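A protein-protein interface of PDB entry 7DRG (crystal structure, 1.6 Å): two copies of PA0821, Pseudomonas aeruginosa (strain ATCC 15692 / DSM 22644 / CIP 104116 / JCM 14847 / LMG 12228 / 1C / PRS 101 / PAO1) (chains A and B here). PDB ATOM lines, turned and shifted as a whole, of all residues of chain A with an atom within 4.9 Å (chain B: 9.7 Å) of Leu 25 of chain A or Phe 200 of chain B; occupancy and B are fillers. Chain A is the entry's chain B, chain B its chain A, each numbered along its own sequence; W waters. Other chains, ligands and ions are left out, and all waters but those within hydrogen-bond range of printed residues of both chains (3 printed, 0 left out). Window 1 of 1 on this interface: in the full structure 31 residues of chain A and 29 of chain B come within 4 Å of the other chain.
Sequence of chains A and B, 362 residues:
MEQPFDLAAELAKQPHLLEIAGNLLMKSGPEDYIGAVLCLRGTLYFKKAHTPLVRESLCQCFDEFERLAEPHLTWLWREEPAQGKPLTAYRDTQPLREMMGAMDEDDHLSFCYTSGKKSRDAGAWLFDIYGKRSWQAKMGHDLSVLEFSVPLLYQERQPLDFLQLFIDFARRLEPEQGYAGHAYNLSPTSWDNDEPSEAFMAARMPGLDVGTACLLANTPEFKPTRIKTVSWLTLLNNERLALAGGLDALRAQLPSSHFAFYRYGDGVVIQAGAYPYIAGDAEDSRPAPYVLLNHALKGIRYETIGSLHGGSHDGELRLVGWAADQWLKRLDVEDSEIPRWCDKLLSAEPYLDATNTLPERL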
ATOM      1  N   PRO A   4      -6.807  -0.625 -19.451  1.00  0.00           N
ATOM      2  CA  PRO A   4      -5.365  -0.433 -19.698  1.00  0.00           C
ATOM      3  C   PRO A   4      -4.493  -0.494 -18.448  1.00  0.00           C
ATOM      4  O   PRO A   4      -3.269  -0.628 -18.585  1.00  0.00           O
ATOM      5  CB  PRO A   4      -5.296   0.960 -20.344  1.00  0.00           C
ATOM      6  CG  PRO A   4      -6.661   1.223 -20.857  1.00  0.00           C
ATOM      7  CD  PRO A   4      -7.571   0.566 -19.870  1.00  0.00           C
ATOM      8  N   LEU A   7      -2.532  -3.806 -17.517  1.00  0.00           N
ATOM      9  CA  LEU A   7      -1.455  -4.012 -18.478  1.00  0.00           C
ATOM     10  C   LEU A   7      -0.307  -3.040 -18.241  1.00  0.00           C
ATOM     11  O   LEU A   7       0.864  -3.411 -18.379  1.00  0.00           O
ATOM     12  CB  LEU A   7      -1.990  -3.876 -19.899  1.00  0.00           C
ATOM     13  CG  LEU A   7      -2.529  -5.169 -20.497  1.00  0.00           C
ATOM     14  CD1 LEU A   7      -3.432  -4.823 -21.657  1.00  0.00           C
ATOM     15  CD2 LEU A   7      -1.380  -6.064 -20.950  1.00  0.00           C
ATOM     16  N   ALA A   8      -0.619  -1.789 -17.893  1.00  0.00           N
ATOM     17  CA  ALA A   8       0.437  -0.838 -17.566  1.00  0.00           C
ATOM     18  C   ALA A   8       1.244  -1.316 -16.367  1.00  0.00           C
ATOM     19  O   ALA A   8       2.469  -1.147 -16.323  1.00  0.00           O
ATOM     20  CB  ALA A   8      -0.159   0.544 -17.296  1.00  0.00           C
ATOM     21  N   LEU A  11       3.456  -4.334 -17.580  1.00  0.00           N
ATOM     22  CA  LEU A  11       4.565  -3.899 -18.425  1.00  0.00           C
ATOM     23  C   LEU A  11       5.654  -3.194 -17.627  1.00  0.00           C
ATOM     24  O   LEU A  11       6.836  -3.286 -17.979  1.00  0.00           O
ATOM     25  CB  LEU A  11       4.045  -2.983 -19.532  1.00  0.00           C
ATOM     26  CG  LEU A  11       3.171  -3.685 -20.568  1.00  0.00           C
ATOM     27  CD1 LEU A  11       2.478  -2.667 -21.459  1.00  0.00           C
ATOM     28  CD2 LEU A  11       4.011  -4.642 -21.394  1.00  0.00           C
ATOM     29  N   ASN A  23      -4.396  -6.405 -32.161  1.00  0.00           N
ATOM     30  CA  ASN A  23      -4.532  -4.976 -32.411  1.00  0.00           C
ATOM     31  C   ASN A  23      -4.299  -4.134 -31.158  1.00  0.00           C
ATOM     32  O   ASN A  23      -4.782  -2.996 -31.081  1.00  0.00           O
ATOM     33  CB  ASN A  23      -5.914  -4.663 -33.012  1.00  0.00           C
ATOM     34  CG  ASN A  23      -5.894  -3.466 -33.929  1.00  0.00           C
ATOM     35  OD1 ASN A  23      -5.074  -3.387 -34.839  1.00  0.00           O
ATOM     36  ND2 ASN A  23      -6.796  -2.517 -33.690  1.00  0.00           N
ATOM     37  N   LEU A  24      -3.558  -4.653 -30.172  1.00  0.00           N
ATOM     38  CA  LEU A  24      -3.459  -3.980 -28.876  1.00  0.00           C
ATOM     39  C   LEU A  24      -2.738  -2.641 -28.977  1.00  0.00           C
ATOM     40  O   LEU A  24      -3.155  -1.659 -28.354  1.00  0.00           O
ATOM     41  CB  LEU A  24      -2.743  -4.875 -27.861  1.00  0.00           C
ATOM     42  CG  LEU A  24      -2.456  -4.212 -26.505  1.00  0.00           C
ATOM     43  CD1 LEU A  24      -3.732  -4.009 -25.707  1.00  0.00           C
ATOM     44  CD2 LEU A  24      -1.447  -5.000 -25.697  1.00  0.00           C
ATOM     45  N   LEU A  25      -1.643  -2.583 -29.731  1.00  0.00           N
ATOM     46  CA  LEU A  25      -0.803  -1.384 -29.779  1.00  0.00           C
ATOM     47  C   LEU A  25      -1.271  -0.421 -30.849  1.00  0.00           C
ATOM     48  O   LEU A  25      -0.472   0.243 -31.522  1.00  0.00           O
ATOM     49  CB  LEU A  25       0.660  -1.773 -29.979  1.00  0.00           C
ATOM     50  CG  LEU A  25       1.523  -2.099 -28.749  1.00  0.00           C
ATOM     51  CD1 LEU A  25       1.787  -0.850 -27.918  1.00  0.00           C
ATOM     52  CD2 LEU A  25       0.909  -3.194 -27.880  1.00  0.00           C
ATOM     53  N   MET A  26      -2.585  -0.349 -31.016  1.00  0.00           N
ATOM     54  CA  MET A  26      -3.231   0.494 -32.003  1.00  0.00           C
ATOM     55  C   MET A  26      -4.098   1.541 -31.322  1.00  0.00           C
ATOM     56  O   MET A  26      -4.453   1.380 -30.160  1.00  0.00           O
ATOM     57  CB  MET A  26      -4.065  -0.360 -32.948  1.00  0.00           C
ATOM     58  CG  MET A  26      -3.297  -0.672 -34.192  1.00  0.00           C
ATOM     59  SD  MET A  26      -2.375   0.978 -34.558  1.00  0.00           S
ATOM     60  CE  MET A  26      -3.194   1.367 -36.273  1.00  0.00           C
ATOM     61  N   LYS A  27      -4.439   2.616 -32.043  1.00  0.00           N
ATOM     62  CA  LYS A  27      -5.347   3.608 -31.473  1.00  0.00           C
ATOM     63  C   LYS A  27      -6.775   3.082 -31.381  1.00  0.00           C
ATOM     64  O   LYS A  27      -7.532   3.506 -30.499  1.00  0.00           O
ATOM     65  CB  LYS A  27      -5.325   4.894 -32.297  1.00  0.00           C
ATOM     66  CG  LYS A  27      -3.942   5.462 -32.553  1.00  0.00           C
ATOM     67  CD  LYS A  27      -3.283   5.971 -31.295  1.00  0.00           C
ATOM     68  CE  LYS A  27      -1.953   6.630 -31.637  1.00  0.00           C
ATOM     69  NZ  LYS A  27      -1.234   7.131 -30.437  1.00  0.00           N
ATOM     70  N   PRO A 196       3.025  -4.038 -34.509  1.00  0.00           N
ATOM     71  CA  PRO A 196       3.378  -3.049 -33.477  1.00  0.00           C
ATOM     72  C   PRO A 196       3.606  -3.659 -32.107  1.00  0.00           C
ATOM     73  O   PRO A 196       4.457  -3.163 -31.355  1.00  0.00           O
ATOM     74  CB  PRO A 196       2.177  -2.094 -33.486  1.00  0.00           C
ATOM     75  CG  PRO A 196       1.627  -2.204 -34.851  1.00  0.00           C
ATOM     76  CD  PRO A 196       1.808  -3.639 -35.244  1.00  0.00           C
ATOM     77  N   SER A 197       2.857  -4.708 -31.752  1.00  0.00           N
ATOM     78  CA  SER A 197       3.108  -5.402 -30.491  1.00  0.00           C
ATOM     79  C   SER A 197       4.503  -6.006 -30.473  1.00  0.00           C
ATOM     80  O   SER A 197       5.213  -5.919 -29.464  1.00  0.00           O
ATOM     81  CB  SER A 197       2.055  -6.487 -30.266  1.00  0.00           C
ATOM     82  OG  SER A 197       0.741  -5.952 -30.286  1.00  0.00           O
ATOM     83  N   PHE A 200       7.111  -3.161 -30.054  1.00  0.00           N
ATOM     84  CA  PHE A 200       7.163  -2.678 -28.678  1.00  0.00           C
ATOM     85  C   PHE A 200       7.942  -3.642 -27.794  1.00  0.00           C
ATOM     86  O   PHE A 200       8.776  -3.228 -26.979  1.00  0.00           O
ATOM     87  CB  PHE A 200       5.731  -2.489 -28.177  1.00  0.00           C
ATOM     88  CG  PHE A 200       5.609  -2.230 -26.706  1.00  0.00           C
ATOM     89  CD1 PHE A 200       6.290  -1.186 -26.103  1.00  0.00           C
ATOM     90  CD2 PHE A 200       4.763  -3.006 -25.935  1.00  0.00           C
ATOM     91  CE1 PHE A 200       6.146  -0.934 -24.745  1.00  0.00           C
ATOM     92  CE2 PHE A 200       4.617  -2.765 -24.581  1.00  0.00           C
ATOM     93  CZ  PHE A 200       5.313  -1.730 -23.984  1.00  0.00           C
ATOM     94  N   GLU A 316       1.333   3.963 -35.436  1.00  0.00           N
ATOM     95  CA  GLU A 316       1.753   2.822 -34.641  1.00  0.00           C
ATOM     96  C   GLU A 316       3.231   2.513 -34.870  1.00  0.00           C
ATOM     97  O   GLU A 316       3.832   2.898 -35.879  1.00  0.00           O
ATOM     98  CB  GLU A 316       0.902   1.595 -34.959  1.00  0.00           C
ATOM     99  CG  GLU A 316       1.181   0.966 -36.304  1.00  0.00           C
ATOM    100  CD  GLU A 316       0.407   1.584 -37.451  1.00  0.00           C
ATOM    101  OE1 GLU A 316      -0.311   2.592 -37.250  1.00  0.00           O
ATOM    102  OE2 GLU A 316       0.517   1.044 -38.571  1.00  0.00           O
ATOM    103  N   ILE B  20       1.049   0.844  -9.172  1.00  0.00           N
ATOM    104  CA  ILE B  20       1.939  -0.195  -9.677  1.00  0.00           C
ATOM    105  C   ILE B  20       2.861  -0.590  -8.533  1.00  0.00           C
ATOM    106  O   ILE B  20       3.511   0.272  -7.930  1.00  0.00           O
ATOM    107  CB  ILE B  20       2.743   0.280 -10.902  1.00  0.00           C
ATOM    108  CG1 ILE B  20       1.794   0.755 -12.005  1.00  0.00           C
ATOM    109  CG2 ILE B  20       3.643  -0.845 -11.430  1.00  0.00           C
ATOM    110  CD1 ILE B  20       2.487   1.327 -13.221  1.00  0.00           C
ATOM    111  N   TYR B 184       1.868   9.259 -13.865  1.00  0.00           N
ATOM    112  CA  TYR B 184       2.261   8.392 -12.760  1.00  0.00           C
ATOM    113  C   TYR B 184       3.357   9.060 -11.942  1.00  0.00           C
ATOM    114  O   TYR B 184       4.442   9.340 -12.466  1.00  0.00           O
ATOM    115  CB  TYR B 184       2.768   7.045 -13.265  1.00  0.00           C
ATOM    116  CG  TYR B 184       1.691   6.072 -13.667  1.00  0.00           C
ATOM    117  CD1 TYR B 184       0.997   5.335 -12.711  1.00  0.00           C
ATOM    118  CD2 TYR B 184       1.373   5.875 -15.003  1.00  0.00           C
ATOM    119  CE1 TYR B 184       0.008   4.435 -13.083  1.00  0.00           C
ATOM    120  CE2 TYR B 184       0.392   4.978 -15.380  1.00  0.00           C
ATOM    121  CZ  TYR B 184      -0.284   4.262 -14.418  1.00  0.00           C
ATOM    122  OH  TYR B 184      -1.260   3.368 -14.801  1.00  0.00           O
ATOM    123  N   GLU B 195      10.414   0.028 -16.522  1.00  0.00           N
ATOM    124  CA  GLU B 195      10.356   0.515 -17.890  1.00  0.00           C
ATOM    125  C   GLU B 195       9.139   1.416 -18.067  1.00  0.00           C
ATOM    126  O   GLU B 195       8.036   1.055 -17.631  1.00  0.00           O
ATOM    127  CB  GLU B 195      10.285  -0.656 -18.879  1.00  0.00           C
ATOM    128  CG  GLU B 195      11.384  -1.692 -18.675  1.00  0.00           C
ATOM    129  CD  GLU B 195      10.881  -3.136 -18.727  1.00  0.00           C
ATOM    130  OE1 GLU B 195       9.900  -3.468 -18.022  1.00  0.00           O
ATOM    131  OE2 GLU B 195      11.479  -3.943 -19.473  1.00  0.00           O
ATOM    132  N   PRO B 196       9.310   2.609 -18.636  1.00  0.00           N
ATOM    133  CA  PRO B 196       8.154   3.441 -19.000  1.00  0.00           C
ATOM    134  C   PRO B 196       7.015   2.713 -19.705  1.00  0.00           C
ATOM    135  O   PRO B 196       5.849   2.892 -19.330  1.00  0.00           O
ATOM    136  CB  PRO B 196       8.779   4.489 -19.933  1.00  0.00           C
ATOM    137  CG  PRO B 196      10.268   4.499 -19.613  1.00  0.00           C
ATOM    138  CD  PRO B 196      10.571   3.368 -18.675  1.00  0.00           C
ATOM    139  N   SER B 197       7.335   1.913 -20.732  1.00  0.00           N
ATOM    140  CA  SER B 197       6.352   1.343 -21.664  1.00  0.00           C
ATOM    141  C   SER B 197       5.723   2.445 -22.520  1.00  0.00           C
ATOM    142  O   SER B 197       4.507   2.489 -22.697  1.00  0.00           O
ATOM    143  CB  SER B 197       5.276   0.527 -20.943  1.00  0.00           C
ATOM    144  OG  SER B 197       5.858  -0.380 -20.021  1.00  0.00           O
ATOM    145  N   GLU B 198       6.576   3.319 -23.071  1.00  0.00           N
ATOM    146  CA  GLU B 198       6.091   4.499 -23.789  1.00  0.00           C
ATOM    147  C   GLU B 198       5.161   4.127 -24.937  1.00  0.00           C
ATOM    148  O   GLU B 198       4.149   4.797 -25.161  1.00  0.00           O
ATOM    149  CB  GLU B 198       7.263   5.325 -24.328  1.00  0.00           C
ATOM    150  CG  GLU B 198       8.385   5.567 -23.343  1.00  0.00           C
ATOM    151  CD  GLU B 198       9.555   4.630 -23.572  1.00  0.00           C
ATOM    152  OE1 GLU B 198      10.139   4.661 -24.676  1.00  0.00           O
ATOM    153  OE2 GLU B 198       9.880   3.847 -22.660  1.00  0.00           O
ATOM    154  N   ALA B 199       5.489   3.071 -25.687  1.00  0.00           N
ATOM    155  CA  ALA B 199       4.657   2.728 -26.834  1.00  0.00           C
ATOM    156  C   ALA B 199       3.274   2.261 -26.404  1.00  0.00           C
ATOM    157  O   ALA B 199       2.297   2.487 -27.127  1.00  0.00           O
ATOM    158  CB  ALA B 199       5.335   1.660 -27.693  1.00  0.00           C
ATOM    159  N   PHE B 200       3.167   1.618 -25.237  1.00  0.00           N
ATOM    160  CA  PHE B 200       1.850   1.224 -24.751  1.00  0.00           C
ATOM    161  C   PHE B 200       1.052   2.443 -24.320  1.00  0.00           C
ATOM    162  O   PHE B 200      -0.134   2.566 -24.647  1.00  0.00           O
ATOM    163  CB  PHE B 200       1.979   0.242 -23.590  1.00  0.00           C
ATOM    164  CG  PHE B 200       0.660  -0.180 -23.022  1.00  0.00           C
ATOM    165  CD1 PHE B 200      -0.098  -1.154 -23.652  1.00  0.00           C
ATOM    166  CD2 PHE B 200       0.174   0.398 -21.863  1.00  0.00           C
ATOM    167  CE1 PHE B 200      -1.320  -1.545 -23.133  1.00  0.00           C
ATOM    168  CE2 PHE B 200      -1.046   0.015 -21.342  1.00  0.00           C
ATOM    169  CZ  PHE B 200      -1.795  -0.958 -21.979  1.00  0.00           C
ATOM    170  N   MET B 201       1.694   3.351 -23.598  1.00  0.00           N
ATOM    171  CA  MET B 201       1.072   4.602 -23.182  1.00  0.00           C
ATOM    172  C   MET B 201       0.602   5.384 -24.389  1.00  0.00           C
ATOM    173  O   MET B 201      -0.523   5.900 -24.410  1.00  0.00           O
ATOM    174  CB  MET B 201       2.062   5.427 -22.363  1.00  0.00           C
ATOM    175  CG  MET B 201       2.682   4.624 -21.250  1.00  0.00           C
ATOM    176  SD  MET B 201       1.312   4.182 -19.965  1.00  0.00           S
ATOM    177  CE  MET B 201       1.807   5.548 -18.677  1.00  0.00           C
ATOM    178  N   ALA B 202       1.455   5.460 -25.413  1.00  0.00           N
ATOM    179  CA  ALA B 202       1.080   6.189 -26.624  1.00  0.00           C
ATOM    180  C   ALA B 202      -0.152   5.585 -27.293  1.00  0.00           C
ATOM    181  O   ALA B 202      -0.983   6.305 -27.858  1.00  0.00           O
ATOM    182  CB  ALA B 202       2.255   6.220 -27.600  1.00  0.00           C
ATOM    183  N   ALA B 203      -0.290   4.262 -27.237  1.00  0.00           N
ATOM    184  CA  ALA B 203      -1.365   3.597 -27.956  1.00  0.00           C
ATOM    185  C   ALA B 203      -2.663   3.576 -27.156  1.00  0.00           C
ATOM    186  O   ALA B 203      -3.746   3.782 -27.716  1.00  0.00           O
ATOM    187  CB  ALA B 203      -0.926   2.169 -28.305  1.00  0.00           C
ATOM    188  N   ARG B 204      -2.567   3.330 -25.849  1.00  0.00           N
ATOM    189  CA  ARG B 204      -3.715   3.026 -25.004  1.00  0.00           C
ATOM    190  C   ARG B 204      -4.024   4.097 -23.973  1.00  0.00           C
ATOM    191  O   ARG B 204      -5.165   4.174 -23.523  1.00  0.00           O
ATOM    192  CB  ARG B 204      -3.492   1.700 -24.263  1.00  0.00           C
ATOM    193  CG  ARG B 204      -3.586   0.430 -25.120  1.00  0.00           C
ATOM    194  CD  ARG B 204      -5.040   0.129 -25.469  1.00  0.00           C
ATOM    195  NE  ARG B 204      -5.397   0.839 -26.683  1.00  0.00           N
ATOM    196  CZ  ARG B 204      -6.617   1.243 -27.013  1.00  0.00           C
ATOM    197  NH1 ARG B 204      -7.654   1.008 -26.219  1.00  0.00           N
ATOM    198  NH2 ARG B 204      -6.788   1.890 -28.154  1.00  0.00           N
ATOM    199  N   MET B 205      -3.039   4.889 -23.557  1.00  0.00           N
ATOM    200  CA  MET B 205      -3.276   5.962 -22.580  1.00  0.00           C
ATOM    201  C   MET B 205      -2.630   7.270 -23.043  1.00  0.00           C
ATOM    202  O   MET B 205      -1.778   7.820 -22.343  1.00  0.00           O
ATOM    203  CB  MET B 205      -2.729   5.568 -21.200  1.00  0.00           C
ATOM    204  CG  MET B 205      -3.239   4.230 -20.672  1.00  0.00           C
ATOM    205  SD  MET B 205      -2.323   3.610 -19.039  1.00  0.00           S
ATOM    206  CE  MET B 205      -3.271   4.700 -17.732  1.00  0.00           C
ATOM    207  N   PRO B 206      -3.017   7.764 -24.225  1.00  0.00           N
ATOM    208  CA  PRO B 206      -2.258   8.866 -24.833  1.00  0.00           C
ATOM    209  C   PRO B 206      -2.438  10.192 -24.124  1.00  0.00           C
ATOM    210  O   PRO B 206      -1.657  11.116 -24.381  1.00  0.00           O
ATOM    211  CB  PRO B 206      -2.796   8.915 -26.270  1.00  0.00           C
ATOM    212  CG  PRO B 206      -4.149   8.336 -26.191  1.00  0.00           C
ATOM    213  CD  PRO B 206      -4.140   7.324 -25.079  1.00  0.00           C
ATOM    214  N   GLY B 207      -3.421  10.309 -23.237  1.00  0.00           N
ATOM    215  CA  GLY B 207      -3.550  11.493 -22.409  1.00  0.00           C
ATOM    216  C   GLY B 207      -2.583  11.570 -21.253  1.00  0.00           C
ATOM    217  O   GLY B 207      -2.533  12.589 -20.565  1.00  0.00           O
ATOM    218  N   LEU B 208      -1.781  10.538 -21.013  1.00  0.00           N
ATOM    219  CA  LEU B 208      -0.854  10.548 -19.893  1.00  0.00           C
ATOM    220  C   LEU B 208       0.455  11.214 -20.279  1.00  0.00           C
ATOM    221  O   LEU B 208       0.979  11.006 -21.380  1.00  0.00           O
ATOM    222  CB  LEU B 208      -0.577   9.126 -19.412  1.00  0.00           C
ATOM    223  CG  LEU B 208      -1.382   8.763 -18.166  1.00  0.00           C
ATOM    224  CD1 LEU B 208      -2.842   8.548 -18.540  1.00  0.00           C
ATOM    225  CD2 LEU B 208      -0.811   7.543 -17.514  1.00  0.00           C
ATOM    226  N   VAL B 210       4.471  11.358 -19.675  1.00  0.00           N
ATOM    227  CA  VAL B 210       5.437  10.281 -19.572  1.00  0.00           C
ATOM    228  C   VAL B 210       6.812  10.941 -19.519  1.00  0.00           C
ATOM    229  O   VAL B 210       7.153  11.739 -20.401  1.00  0.00           O
ATOM    230  CB  VAL B 210       5.248   9.330 -20.776  1.00  0.00           C
ATOM    231  CG1 VAL B 210       6.517   8.891 -21.433  1.00  0.00           C
ATOM    232  CG2 VAL B 210       4.320   8.162 -20.415  1.00  0.00           C
ATOM    233  N   ILE B 278      -7.554  10.488 -19.744  1.00  0.00           N
ATOM    234  CA  ILE B 278      -6.573   9.415 -19.899  1.00  0.00           C
ATOM    235  C   ILE B 278      -6.536   8.933 -21.342  1.00  0.00           C
ATOM    236  O   ILE B 278      -5.465   8.732 -21.933  1.00  0.00           O
ATOM    237  CB  ILE B 278      -6.910   8.246 -18.952  1.00  0.00           C
ATOM    238  CG1 ILE B 278      -6.662   8.620 -17.497  1.00  0.00           C
ATOM    239  CG2 ILE B 278      -6.125   7.000 -19.349  1.00  0.00           C
ATOM    240  CD1 ILE B 278      -7.142   7.562 -16.508  1.00  0.00           C
ATOM    241  N   ALA B 279      -7.714   8.717 -21.912  1.00  0.00           N
ATOM    242  CA  ALA B 279      -7.863   8.174 -23.247  1.00  0.00           C
ATOM    243  C   ALA B 279      -9.185   8.674 -23.807  1.00  0.00           C
ATOM    244  O   ALA B 279      -9.895   9.459 -23.172  1.00  0.00           O
ATOM    245  CB  ALA B 279      -7.795   6.643 -23.235  1.00  0.00           C
ATOM    246  N   SER B 285      -8.372   5.793 -28.970  1.00  0.00           N
ATOM    247  CA  SER B 285      -7.862   6.096 -27.641  1.00  0.00           C
ATOM    248  C   SER B 285      -7.475   7.562 -27.471  1.00  0.00           C
ATOM    249  O   SER B 285      -7.337   8.020 -26.334  1.00  0.00           O
ATOM    250  CB  SER B 285      -6.656   5.206 -27.330  1.00  0.00           C
ATOM    251  OG  SER B 285      -5.578   5.509 -28.194  1.00  0.00           O
ATOM    252  N   ALA B 323      11.685   4.993 -29.482  1.00  0.00           N
ATOM    253  CA  ALA B 323      10.304   4.874 -29.022  1.00  0.00           C
ATOM    254  C   ALA B 323       9.837   6.154 -28.339  1.00  0.00           C
ATOM    255  O   ALA B 323       8.668   6.536 -28.455  1.00  0.00           O
ATOM    256  CB  ALA B 323      10.160   3.683 -28.074  1.00  0.00           C
ATOM    257  N   ALA B 324      10.737   6.825 -27.617  1.00  0.00           N
ATOM    258  CA  ALA B 324      10.372   8.075 -26.958  1.00  0.00           C
ATOM    259  C   ALA B 324      10.039   9.161 -27.975  1.00  0.00           C
ATOM    260  O   ALA B 324       9.066   9.908 -27.801  1.00  0.00           O
ATOM    261  CB  ALA B 324      11.504   8.518 -26.037  1.00  0.00           C
ATOM    262  N   GLN B 326       8.819   8.629 -30.868  1.00  0.00           N
ATOM    263  CA  GLN B 326       7.508   8.245 -31.386  1.00  0.00           C
ATOM    264  C   GLN B 326       6.391   8.679 -30.441  1.00  0.00           C
ATOM    265  O   GLN B 326       5.307   9.079 -30.886  1.00  0.00           O
ATOM    266  CB  GLN B 326       7.454   6.732 -31.602  1.00  0.00           C
ATOM    267  CG  GLN B 326       8.343   6.221 -32.720  1.00  0.00           C
ATOM    268  CD  GLN B 326       7.843   6.648 -34.084  1.00  0.00           C
ATOM    269  OE1 GLN B 326       6.829   6.142 -34.575  1.00  0.00           O
ATOM    270  NE2 GLN B 326       8.543   7.591 -34.701  1.00  0.00           N
ATOM    271  N   TRP B 327       6.633   8.580 -29.130  1.00  0.00           N
ATOM    272  CA  TRP B 327       5.610   8.935 -28.152  1.00  0.00           C
ATOM    273  C   TRP B 327       5.188  10.392 -28.294  1.00  0.00           C
ATOM    274  O   TRP B 327       4.016  10.724 -28.074  1.00  0.00           O
ATOM    275  CB  TRP B 327       6.130   8.658 -26.737  1.00  0.00           C
ATOM    276  CG  TRP B 327       5.188   9.090 -25.645  1.00  0.00           C
ATOM    277  CD1 TRP B 327       4.192   8.351 -25.074  1.00  0.00           C
ATOM    278  CD2 TRP B 327       5.145  10.377 -25.015  1.00  0.00           C
ATOM    279  NE1 TRP B 327       3.533   9.103 -24.122  1.00  0.00           N
ATOM    280  CE2 TRP B 327       4.098  10.348 -24.072  1.00  0.00           C
ATOM    281  CE3 TRP B 327       5.894  11.549 -25.155  1.00  0.00           C
ATOM    282  CZ2 TRP B 327       3.780  11.454 -23.269  1.00  0.00           C
ATOM    283  CZ3 TRP B 327       5.575  12.647 -24.362  1.00  0.00           C
ATOM    284  CH2 TRP B 327       4.530  12.587 -23.432  1.00  0.00           C
ATOM    285  N   ARG B 330       2.022  10.927 -30.445  1.00  0.00           N
ATOM    286  CA  ARG B 330       0.915  10.005 -30.201  1.00  0.00           C
ATOM    287  C   ARG B 330      -0.458  10.626 -30.426  1.00  0.00           C
ATOM    288  O   ARG B 330      -1.419   9.890 -30.667  1.00  0.00           O
ATOM    289  CB  ARG B 330       0.998   9.459 -28.775  1.00  0.00           C
ATOM    290  CG  ARG B 330       0.650  10.490 -27.715  1.00  0.00           C
ATOM    291  CD  ARG B 330       1.265  10.185 -26.353  1.00  0.00           C
ATOM    292  NE  ARG B 330       0.897  11.267 -25.436  1.00  0.00           N
ATOM    293  CZ  ARG B 330       1.475  12.463 -25.421  1.00  0.00           C
ATOM    294  NH1 ARG B 330       2.475  12.733 -26.250  1.00  0.00           N
ATOM    295  NH2 ARG B 330       1.048  13.402 -24.575  1.00  0.00           N
HETATM  296  O   HOH W   1       4.683   4.833 -33.101  1.00  0.00           O
HETATM  297  O   HOH W   2       6.535   3.696 -36.180  1.00  0.00           O
HETATM  298  O   HOH W   3       4.108   0.370 -17.707  1.00  0.00           O
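O of Ala 202 of chain B sits at hydrogen-bond distance from NZ of Lys 27 of chain A (2.7 Å). NH2 of Arg 204 of chain B lies within hydrogen-bond range of O of Met 26 of chain A. O of Lys 27 of chain A is in hydrogen-bond range of NH2 of Arg 204 of chain B, at 2.9 Å. The backbone NH of Ser 285 of chain B lies within hydrogen-bond range of the backbone carbonyl oxygen of Lys 27 of chain A, 2.9 Å away. The backbone carbonyl oxygen (O) of Arg 330 of chain B lies within hydrogen-bond range of the side-chain amino group (NZ) of Lys 27 of chain A. OE1 of Glu 195 of chain B lies close to O of Leu 11 of chain A (3.1 Å). O of Met 26 of chain A lies close to O of Ala 203 of chain B, at 3.5 Å.
Water W3 lies within hydrogen-bond range of O of Ala 8 of chain A (2.6 Å), OG of Ser 197 of chain B (3.0 Å) and O of Pro 196 of chain B (3.5 Å). Water W2 lies within hydrogen-bond range of O of Glu 316 of chain A (2.8 Å) and OE1 of Gln 326 of chain B (2.9 Å). Water W1 bridges OE1 of Gln 326 of chain B and O of Glu 316 of chain A.
Of chain B, only Ala 199, Phe 200 and Ala 203 come within 4 Å of Leu 25 of chain A. Phe 200 of chain B touches six residues of chain A. Of the printed residues of chain B, Leu 7 of chain A touches Phe 200 (3.6 Å). Leu 24 of chain A touches one residue of chain B. No residue of chain B comes within 4 Å of Ser 197 of chain A. Of the printed residues of chain A, Arg 204 of chain B touches Leu 24, Met 26 and Lys 27. Of the printed residues of chain A, Ile 20 of chain B touches Ala 8. Val 210 of chain B touches none of the printed residues of chain A. Met 201 of chain B touches none of the printed residues of chain A.
Phe 200 of chain A touches Ser 197 of chain B, but with the chains exchanged Ser 197 of chain A does not touch Phe 200 of chain B (8.2 Å). Phe 200 of chain B touches its own counterpart, Phe 200 of chain A.
Pro 4 of chain A touches Phe 200 of chain B (O to CE2, 3.6 Å). CB of Pro 4 of chain A touches CG of Met 205 of chain B, at 3.9 Å. Ala 8 of chain A touches Ile 20 of chain B (O to CD1, 3.97 Å). Ala 8 of chain A touches Phe 200 of chain B (N to CE2, 3.9 Å). OG of Ser 197 of chain B touches CB of Leu 11 of chain A (3.2 Å). Leu 24 of chain A touches Arg 204 of chain B. Leu 25 of chain A touches Ala 203 of chain B (C to CB, 3.6 Å).
Of the 13 printed residues of chain A, 9 touch a printed residue of chain B. Hydrophobic or aromatic side chains of chain A within 4 Å of the printed part of chain B: Pro 4, Leu 7, Ala 8, Leu 11, Leu 25 and Phe 200. Among the printed residues, no Asp or Glu carboxylate lies within 4 Å of a Lys or Arg side-chain nitrogen of the other chain.
The backbone carbonyl oxygen (O) of Ala 203 of chain B lies within hydrogen-bond range of the side-chain hydroxyl (OG) of Ser 285 of chain B, at 2.6 Å. NE of Arg 330 of chain B lies within hydrogen-bond range of O of Pro 206 of chain B. The backbone carbonyl oxygen (O) of Trp 327 of chain B is in hydrogen-bond range of the guanidinium group (NH1) of Arg 330 of chain B.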
